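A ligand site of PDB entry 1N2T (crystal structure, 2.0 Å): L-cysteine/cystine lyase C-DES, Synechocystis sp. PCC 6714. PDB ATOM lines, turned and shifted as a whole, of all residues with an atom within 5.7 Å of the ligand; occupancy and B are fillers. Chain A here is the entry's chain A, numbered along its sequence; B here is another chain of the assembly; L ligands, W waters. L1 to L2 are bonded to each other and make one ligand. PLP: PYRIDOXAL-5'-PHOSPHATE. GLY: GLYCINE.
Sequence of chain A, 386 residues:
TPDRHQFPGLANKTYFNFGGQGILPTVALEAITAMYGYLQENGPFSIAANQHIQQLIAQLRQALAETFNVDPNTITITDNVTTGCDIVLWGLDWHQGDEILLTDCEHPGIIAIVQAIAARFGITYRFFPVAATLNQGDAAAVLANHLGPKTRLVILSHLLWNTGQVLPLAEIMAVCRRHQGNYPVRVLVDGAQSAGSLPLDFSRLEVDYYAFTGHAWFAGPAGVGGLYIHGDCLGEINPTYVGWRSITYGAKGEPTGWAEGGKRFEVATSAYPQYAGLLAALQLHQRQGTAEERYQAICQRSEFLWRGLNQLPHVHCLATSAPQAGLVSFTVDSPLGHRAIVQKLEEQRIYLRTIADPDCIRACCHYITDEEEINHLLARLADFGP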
ATOM      1  N   GLY A  19       4.773  23.006  35.839  1.00  0.00           N
ATOM      2  CA  GLY A  19       5.346  22.241  34.743  1.00  0.00           C
ATOM      3  C   GLY A  19       4.665  22.510  33.410  1.00  0.00           C
ATOM      4  O   GLY A  19       5.263  22.269  32.364  1.00  0.00           O
ATOM      5  N   GLY A  20       3.412  22.965  33.470  1.00  0.00           N
ATOM      6  CA  GLY A  20       2.624  23.297  32.292  1.00  0.00           C
ATOM      7  C   GLY A  20       2.976  24.733  31.923  1.00  0.00           C
ATOM      8  O   GLY A  20       3.386  25.025  30.806  1.00  0.00           O
ATOM      9  N   ASP A  79      10.938  29.983  20.563  1.00  0.00           N
ATOM     10  CA  ASP A  79       9.632  30.302  21.143  1.00  0.00           C
ATOM     11  C   ASP A  79       9.192  29.250  22.163  1.00  0.00           C
ATOM     12  O   ASP A  79       8.300  29.518  22.959  1.00  0.00           O
ATOM     13  CB  ASP A  79       8.551  30.336  20.053  1.00  0.00           C
ATOM     14  CG  ASP A  79       8.824  31.368  18.985  1.00  0.00           C
ATOM     15  OD1 ASP A  79       8.328  31.177  17.856  1.00  0.00           O
ATOM     16  OD2 ASP A  79       9.509  32.366  19.268  1.00  0.00           O
ATOM     17  N   ASN A  80       9.817  28.079  22.147  1.00  0.00           N
ATOM     18  CA  ASN A  80       9.388  27.008  23.043  1.00  0.00           C
ATOM     19  C   ASN A  80      10.405  25.862  22.996  1.00  0.00           C
ATOM     20  O   ASN A  80      11.366  25.911  22.236  1.00  0.00           O
ATOM     21  CB  ASN A  80       8.036  26.497  22.559  1.00  0.00           C
ATOM     22  CG  ASN A  80       8.001  26.267  21.044  1.00  0.00           C
ATOM     23  OD1 ASN A  80       8.845  25.556  20.501  1.00  0.00           O
ATOM     24  ND2 ASN A  80       7.007  26.856  20.356  1.00  0.00           N
ATOM     25  N   VAL A  81      10.156  24.812  23.775  1.00  0.00           N
ATOM     26  CA  VAL A  81      11.045  23.644  23.797  1.00  0.00           C
ATOM     27  C   VAL A  81      11.102  22.923  22.437  1.00  0.00           C
ATOM     28  O   VAL A  81      12.179  22.582  21.920  1.00  0.00           O
ATOM     29  CB  VAL A  81      10.566  22.593  24.839  1.00  0.00           C
ATOM     30  CG1 VAL A  81      11.474  21.369  24.787  1.00  0.00           C
ATOM     31  CG2 VAL A  81      10.558  23.178  26.243  1.00  0.00           C
ATOM     32  N   THR A  82       9.934  22.690  21.862  1.00  0.00           N
ATOM     33  CA  THR A  82       9.828  21.946  20.615  1.00  0.00           C
ATOM     34  C   THR A  82      10.665  22.474  19.465  1.00  0.00           C
ATOM     35  O   THR A  82      11.317  21.682  18.772  1.00  0.00           O
ATOM     36  CB  THR A  82       8.364  21.815  20.198  1.00  0.00           C
ATOM     37  OG1 THR A  82       7.660  21.166  21.264  1.00  0.00           O
ATOM     38  CG2 THR A  82       8.230  20.972  18.909  1.00  0.00           C
ATOM     39  N   THR A  83      10.654  23.783  19.252  1.00  0.00           N
ATOM     40  CA  THR A  83      11.431  24.383  18.162  1.00  0.00           C
ATOM     41  C   THR A  83      12.923  24.045  18.262  1.00  0.00           C
ATOM     42  O   THR A  83      13.571  23.801  17.239  1.00  0.00           O
ATOM     43  CB  THR A  83      11.230  25.920  18.141  1.00  0.00           C
ATOM     44  OG1 THR A  83       9.846  26.186  17.897  1.00  0.00           O
ATOM     45  CG2 THR A  83      12.084  26.573  17.009  1.00  0.00           C
ATOM     46  N   GLU A 106       8.993  10.082  26.052  1.00  0.00           N
ATOM     47  CA  GLU A 106       9.153  11.340  25.354  1.00  0.00           C
ATOM     48  C   GLU A 106       7.803  11.935  24.948  1.00  0.00           C
ATOM     49  O   GLU A 106       6.798  11.240  24.857  1.00  0.00           O
ATOM     50  CB  GLU A 106      10.064  11.161  24.138  1.00  0.00           C
ATOM     51  CG  GLU A 106      11.485  10.705  24.517  1.00  0.00           C
ATOM     52  CD  GLU A 106      12.035  11.490  25.717  1.00  0.00           C
ATOM     53  OE1 GLU A 106      11.950  12.735  25.719  1.00  0.00           O
ATOM     54  OE2 GLU A 106      12.560  10.853  26.666  1.00  0.00           O
ATOM     55  N   HIS A 107       7.811  13.231  24.714  1.00  0.00           N
ATOM     56  CA  HIS A 107       6.610  13.985  24.367  1.00  0.00           C
ATOM     57  C   HIS A 107       6.084  13.645  22.963  1.00  0.00           C
ATOM     58  O   HIS A 107       6.862  13.472  22.020  1.00  0.00           O
ATOM     59  CB  HIS A 107       6.950  15.487  24.481  1.00  0.00           C
ATOM     60  CG  HIS A 107       5.766  16.373  24.732  1.00  0.00           C
ATOM     61  ND1 HIS A 107       5.151  17.095  23.737  1.00  0.00           N
ATOM     62  CD2 HIS A 107       5.096  16.646  25.879  1.00  0.00           C
ATOM     63  CE1 HIS A 107       4.143  17.780  24.256  1.00  0.00           C
ATOM     64  NE2 HIS A 107       4.089  17.528  25.557  1.00  0.00           N
ATOM     65  N   ILE A 110       7.507  15.583  20.057  1.00  0.00           N
ATOM     66  CA  ILE A 110       8.878  15.222  19.696  1.00  0.00           C
ATOM     67  C   ILE A 110       8.864  13.965  18.804  1.00  0.00           C
ATOM     68  O   ILE A 110       9.544  13.896  17.786  1.00  0.00           O
ATOM     69  CB  ILE A 110       9.711  14.962  20.976  1.00  0.00           C
ATOM     70  CG1 ILE A 110       9.683  16.193  21.885  1.00  0.00           C
ATOM     71  CG2 ILE A 110      11.125  14.566  20.621  1.00  0.00           C
ATOM     72  CD1 ILE A 110       9.785  17.526  21.176  1.00  0.00           C
ATOM     73  N   SER A 157      14.408  12.951  27.763  1.00  0.00           N
ATOM     74  CA  SER A 157      14.003  14.082  28.614  1.00  0.00           C
ATOM     75  C   SER A 157      14.817  13.938  29.915  1.00  0.00           C
ATOM     76  O   SER A 157      14.820  12.865  30.529  1.00  0.00           O
ATOM     77  CB  SER A 157      12.503  13.994  28.915  1.00  0.00           C
ATOM     78  OG  SER A 157      11.734  14.320  27.759  1.00  0.00           O
ATOM     79  N   LEU A 159      14.330  15.344  32.867  1.00  0.00           N
ATOM     80  CA  LEU A 159      13.376  15.101  33.952  1.00  0.00           C
ATOM     81  C   LEU A 159      12.101  14.675  33.216  1.00  0.00           C
ATOM     82  O   LEU A 159      11.570  15.442  32.419  1.00  0.00           O
ATOM     83  CB  LEU A 159      13.143  16.371  34.782  1.00  0.00           C
ATOM     84  CG  LEU A 159      11.974  16.445  35.776  1.00  0.00           C
ATOM     85  CD1 LEU A 159      11.974  15.253  36.704  1.00  0.00           C
ATOM     86  CD2 LEU A 159      12.097  17.752  36.568  1.00  0.00           C
ATOM     87  N   TRP A 161       8.439  14.075  32.170  1.00  0.00           N
ATOM     88  CA  TRP A 161       7.189  14.813  32.359  1.00  0.00           C
ATOM     89  C   TRP A 161       6.051  13.957  32.881  1.00  0.00           C
ATOM     90  O   TRP A 161       5.103  14.489  33.456  1.00  0.00           O
ATOM     91  CB  TRP A 161       6.747  15.466  31.038  1.00  0.00           C
ATOM     92  CG  TRP A 161       6.092  14.498  30.048  1.00  0.00           C
ATOM     93  CD1 TRP A 161       6.585  13.289  29.633  1.00  0.00           C
ATOM     94  CD2 TRP A 161       4.857  14.689  29.346  1.00  0.00           C
ATOM     95  NE1 TRP A 161       5.732  12.719  28.710  1.00  0.00           N
ATOM     96  CE2 TRP A 161       4.665  13.548  28.510  1.00  0.00           C
ATOM     97  CE3 TRP A 161       3.900  15.715  29.321  1.00  0.00           C
ATOM     98  CZ2 TRP A 161       3.556  13.411  27.674  1.00  0.00           C
ATOM     99  CZ3 TRP A 161       2.795  15.571  28.479  1.00  0.00           C
ATOM    100  CH2 TRP A 161       2.629  14.423  27.672  1.00  0.00           C
ATOM    101  N   ASP A 190      15.701  16.896  25.970  1.00  0.00           N
ATOM    102  CA  ASP A 190      14.499  17.725  26.085  1.00  0.00           C
ATOM    103  C   ASP A 190      14.498  18.198  27.561  1.00  0.00           C
ATOM    104  O   ASP A 190      14.268  17.407  28.476  1.00  0.00           O
ATOM    105  CB  ASP A 190      13.256  16.884  25.785  1.00  0.00           C
ATOM    106  CG  ASP A 190      11.950  17.644  25.975  1.00  0.00           C
ATOM    107  OD1 ASP A 190      10.959  17.304  25.280  1.00  0.00           O
ATOM    108  OD2 ASP A 190      11.896  18.554  26.834  1.00  0.00           O
ATOM    109  N   ALA A 192      12.365  20.389  29.052  1.00  0.00           N
ATOM    110  CA  ALA A 192      11.130  21.112  29.374  1.00  0.00           C
ATOM    111  C   ALA A 192      10.846  21.195  30.863  1.00  0.00           C
ATOM    112  O   ALA A 192      10.306  22.177  31.342  1.00  0.00           O
ATOM    113  CB  ALA A 192       9.946  20.467  28.675  1.00  0.00           C
ATOM    114  N   GLN A 193      11.190  20.144  31.601  1.00  0.00           N
ATOM    115  CA  GLN A 193      10.944  20.107  33.037  1.00  0.00           C
ATOM    116  C   GLN A 193      12.189  20.422  33.867  1.00  0.00           C
ATOM    117  O   GLN A 193      12.088  21.041  34.936  1.00  0.00           O
ATOM    118  CB  GLN A 193      10.415  18.728  33.431  1.00  0.00           C
ATOM    119  CG  GLN A 193       9.131  18.324  32.749  1.00  0.00           C
ATOM    120  CD  GLN A 193       7.996  19.276  33.044  1.00  0.00           C
ATOM    121  OE1 GLN A 193       7.894  19.854  34.144  1.00  0.00           O
ATOM    122  NE2 GLN A 193       7.123  19.468  32.057  1.00  0.00           N
ATOM    123  N   THR A 213      12.509  25.753  27.486  1.00  0.00           N
ATOM    124  CA  THR A 213      11.564  26.850  27.317  1.00  0.00           C
ATOM    125  C   THR A 213      11.634  27.769  28.533  1.00  0.00           C
ATOM    126  O   THR A 213      12.156  27.396  29.596  1.00  0.00           O
ATOM    127  CB  THR A 213      10.093  26.372  27.155  1.00  0.00           C
ATOM    128  OG1 THR A 213       9.275  27.484  26.767  1.00  0.00           O
ATOM    129  CG2 THR A 213       9.527  25.801  28.489  1.00  0.00           C
ATOM    130  N   HIS A 215       8.759  29.447  29.689  1.00  0.00           N
ATOM    131  CA  HIS A 215       7.446  29.618  30.303  1.00  0.00           C
ATOM    132  C   HIS A 215       6.999  28.645  31.379  1.00  0.00           C
ATOM    133  O   HIS A 215       5.922  28.827  31.948  1.00  0.00           O
ATOM    134  CB  HIS A 215       6.348  29.697  29.214  1.00  0.00           C
ATOM    135  CG  HIS A 215       5.930  28.372  28.656  1.00  0.00           C
ATOM    136  ND1 HIS A 215       6.686  27.681  27.730  1.00  0.00           N
ATOM    137  CD2 HIS A 215       4.835  27.621  28.878  1.00  0.00           C
ATOM    138  CE1 HIS A 215       6.069  26.557  27.406  1.00  0.00           C
ATOM    139  NE2 HIS A 215       4.938  26.491  28.095  1.00  0.00           N
ATOM    140  N   ARG A 353      -2.731  18.239  36.782  1.00  0.00           N
ATOM    141  CA  ARG A 353      -3.018  17.773  35.430  1.00  0.00           C
ATOM    142  C   ARG A 353      -3.004  16.262  35.297  1.00  0.00           C
ATOM    143  O   ARG A 353      -2.366  15.533  36.077  1.00  0.00           O
ATOM    144  CB  ARG A 353      -2.031  18.358  34.393  1.00  0.00           C
ATOM    145  CG  ARG A 353      -0.709  17.632  34.295  1.00  0.00           C
ATOM    146  CD  ARG A 353      -0.014  17.924  32.975  1.00  0.00           C
ATOM    147  NE  ARG A 353      -0.650  17.225  31.849  1.00  0.00           N
ATOM    148  CZ  ARG A 353      -0.365  17.437  30.562  1.00  0.00           C
ATOM    149  NH1 ARG A 353       0.555  18.347  30.210  1.00  0.00           N
ATOM    150  NH2 ARG A 353      -0.994  16.745  29.624  1.00  0.00           N
ATOM    151  N   ARG A 362      -0.672  14.417  38.024  1.00  0.00           N
ATOM    152  CA  ARG A 362       0.625  15.006  38.373  1.00  0.00           C
ATOM    153  C   ARG A 362       0.521  16.371  39.029  1.00  0.00           C
ATOM    154  O   ARG A 362      -0.251  17.240  38.587  1.00  0.00           O
ATOM    155  CB  ARG A 362       1.484  15.137  37.109  1.00  0.00           C
ATOM    156  CG  ARG A 362       2.941  15.595  37.319  1.00  0.00           C
ATOM    157  CD  ARG A 362       3.578  16.036  35.968  1.00  0.00           C
ATOM    158  NE  ARG A 362       3.087  17.350  35.530  1.00  0.00           N
ATOM    159  CZ  ARG A 362       3.360  17.927  34.367  1.00  0.00           C
ATOM    160  NH1 ARG A 362       4.131  17.337  33.469  1.00  0.00           N
ATOM    161  NH2 ARG A 362       2.925  19.153  34.130  1.00  0.00           N
ATOM    162  N   PHE B  45      -2.053  27.604  33.396  1.00  0.00           N
ATOM    163  CA  PHE B  45      -2.223  26.288  32.753  1.00  0.00           C
ATOM    164  C   PHE B  45      -3.382  25.586  33.474  1.00  0.00           C
ATOM    165  O   PHE B  45      -3.294  25.300  34.678  1.00  0.00           O
ATOM    166  CB  PHE B  45      -0.953  25.422  32.870  1.00  0.00           C
ATOM    167  CG  PHE B  45      -0.973  24.166  32.025  1.00  0.00           C
ATOM    168  CD1 PHE B  45      -0.459  24.174  30.738  1.00  0.00           C
ATOM    169  CD2 PHE B  45      -1.550  22.989  32.503  1.00  0.00           C
ATOM    170  CE1 PHE B  45      -0.489  23.035  29.934  1.00  0.00           C
ATOM    171  CE2 PHE B  45      -1.592  21.837  31.707  1.00  0.00           C
ATOM    172  CZ  PHE B  45      -1.053  21.864  30.416  1.00  0.00           C
ATOM    173  N   TRP B 244       3.399  19.466  19.184  1.00  0.00           N
ATOM    174  CA  TRP B 244       2.107  18.990  19.673  1.00  0.00           C
ATOM    175  C   TRP B 244       0.888  19.660  19.032  1.00  0.00           C
ATOM    176  O   TRP B 244      -0.204  19.095  19.068  1.00  0.00           O
ATOM    177  CB  TRP B 244       1.998  19.106  21.219  1.00  0.00           C
ATOM    178  CG  TRP B 244       2.185  20.478  21.807  1.00  0.00           C
ATOM    179  CD1 TRP B 244       3.379  21.079  22.169  1.00  0.00           C
ATOM    180  CD2 TRP B 244       1.166  21.447  22.083  1.00  0.00           C
ATOM    181  NE1 TRP B 244       3.156  22.346  22.630  1.00  0.00           N
ATOM    182  CE2 TRP B 244       1.804  22.605  22.589  1.00  0.00           C
ATOM    183  CE3 TRP B 244      -0.230  21.455  21.930  1.00  0.00           C
ATOM    184  CZ2 TRP B 244       1.098  23.748  22.959  1.00  0.00           C
ATOM    185  CZ3 TRP B 244      -0.940  22.605  22.306  1.00  0.00           C
ATOM    186  CH2 TRP B 244      -0.265  23.739  22.800  1.00  0.00           C
ATOM    187  N   ALA B 268       4.031  24.712  18.506  1.00  0.00           N
ATOM    188  CA  ALA B 268       3.831  24.526  19.929  1.00  0.00           C
ATOM    189  C   ALA B 268       3.488  25.826  20.659  1.00  0.00           C
ATOM    190  O   ALA B 268       2.863  26.739  20.083  1.00  0.00           O
ATOM    191  CB  ALA B 268       5.090  23.824  20.553  1.00  0.00           C
ATOM    192  N   THR B 269       3.918  25.947  21.926  1.00  0.00           N
ATOM    193  CA  THR B 269       3.545  27.146  22.684  1.00  0.00           C
ATOM    194  C   THR B 269       3.934  28.451  21.998  1.00  0.00           C
ATOM    195  O   THR B 269       5.065  28.613  21.541  1.00  0.00           O
ATOM    196  CB  THR B 269       4.154  27.136  24.138  1.00  0.00           C
ATOM    197  OG1 THR B 269       3.707  25.965  24.844  1.00  0.00           O
ATOM    198  CG2 THR B 269       3.654  28.385  24.915  1.00  0.00           C
HETATM  199  N1  PLP L   1       8.755  18.239  26.164  1.00  0.00           N
HETATM  200  C2  PLP L   1       8.362  17.906  27.447  1.00  0.00           C
HETATM  201  C2A PLP L   1       9.161  16.820  28.204  1.00  0.00           C
HETATM  202  C3  PLP L   1       7.261  18.562  28.001  1.00  0.00           C
HETATM  203  O3  PLP L   1       6.832  18.267  29.299  1.00  0.00           O
HETATM  204  C4  PLP L   1       6.578  19.563  27.226  1.00  0.00           C
HETATM  205  C4A PLP L   1       5.357  20.294  27.826  1.00  0.00           C
HETATM  206  C5  PLP L   1       7.048  19.858  25.890  1.00  0.00           C
HETATM  207  C6  PLP L   1       8.132  19.180  25.401  1.00  0.00           C
HETATM  208  C5A PLP L   1       6.480  20.909  24.915  1.00  0.00           C
HETATM  209  O4P PLP L   1       6.845  22.256  25.129  1.00  0.00           O
HETATM  210  P   PLP L   1       6.513  23.454  24.172  1.00  0.00           P
HETATM  211  O1P PLP L   1       7.340  23.241  22.967  1.00  0.00           O
HETATM  212  O2P PLP L   1       7.264  24.537  25.078  1.00  0.00           O
HETATM  213  O3P PLP L   1       5.069  23.789  24.041  1.00  0.00           O
HETATM  214  N   GLY L   2       4.944  19.966  29.087  1.00  0.00           N
HETATM  215  CA  GLY L   2       3.807  20.630  29.676  1.00  0.00           C
HETATM  216  C   GLY L   2       3.379  19.737  30.825  1.00  0.00           C
HETATM  217  O   GLY L   2       2.394  20.050  31.497  1.00  0.00           O
HETATM  218  OXT GLY L   2       4.069  18.718  31.039  1.00  0.00           O
HETATM  219  O   HOH W   1       6.757  23.287  28.017  1.00  0.00           O
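The side-chain carboxylate of Asp 190 is in hydrogen-bond range of the backbone NH of Ala 192 (2.9 Å). The backbone carbonyl oxygen of Thr 269 of chain B is in hydrogen-bond range of the side-chain amide nitrogen of Asn 80 (2.9 Å). The backbone NH of Thr 82 sits at hydrogen-bond distance from the side-chain amide oxygen of Asn 80 (3.4 Å). The backbone NH (N) of Arg 362 is in hydrogen-bond range of the backbone carbonyl oxygen (O) of Arg 353, at 2.8 Å. The guanidinium group of Arg 362 sits at hydrogen-bond distance from the backbone carbonyl oxygen of Trp 161, at 3.0 Å. The backbone NH (N) of Thr 83 lies within hydrogen-bond range of the side-chain amide oxygen (OD1) of Asn 80 (2.8 Å). The side-chain hydroxyl of Thr 213 sits at hydrogen-bond distance from a ring nitrogen (ND1) of His 215 (2.8 Å). The side-chain hydroxyl (OG) of Ser 157 sits at hydrogen-bond distance from the side-chain carboxylate (OE1) of Glu 106, at 2.6 Å.
A nitrogen (N1) of PLP L1 sits at hydrogen-bond distance from the side-chain carboxylate (OD1) of Asp 190, 2.6 Å away. N of Thr 269 of chain B is in hydrogen-bond range of O3P of PLP L1 (3.2 Å). The side-chain hydroxyl (OG1) of Thr 269 of chain B sits at hydrogen-bond distance from an oxygen (O3P) of PLP L1 (2.7 Å). N of Thr 82 is in hydrogen-bond range of O1P of PLP L1 (2.9 Å). OG1 of Thr 82 lies within hydrogen-bond range of O1P of PLP L1 (2.7 Å). NE1 of Trp 244 of chain B lies within hydrogen-bond range of O3P of PLP L1 (2.8 Å). NH1 of Arg 362 is in salt-bridge range of OXT of GLY L2 (2.8 Å). NH1 of Arg 353 lies within salt-bridge range of O of GLY L2 (2.8 Å). The side-chain amide nitrogen of Gln 193 lies within hydrogen-bond range of an oxygen (O3) of PLP L1 (3.0 Å). The backbone NH (N) of Val 81 lies within hydrogen-bond range of an oxygen (O2P) of PLP L1 (3.2 Å).
Gly 19 touches the ligand. CA of Gly 20 touches O of GLY L2 (3.4 Å). CB of Asn 80 touches O2P of PLP L1 (3.3 Å). CD2 of His 107 touches C4 of PLP L1, 3.5 Å away. OG of Ser 157 touches C2A of PLP L1, 3.6 Å away. CB of Trp 161 touches O3 of PLP L1, 3.3 Å away. Ala 192 touches the ligand. Thr 213 touches the ligand. CE1 of His 215 touches O2P of PLP L1, at 3.3 Å. CB of Ala 268 of chain B touches O1P of PLP L1, 3.4 Å away. The nearest printed residue that does not touch the ligand is Phe 45 of chain B (4.04 Å).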
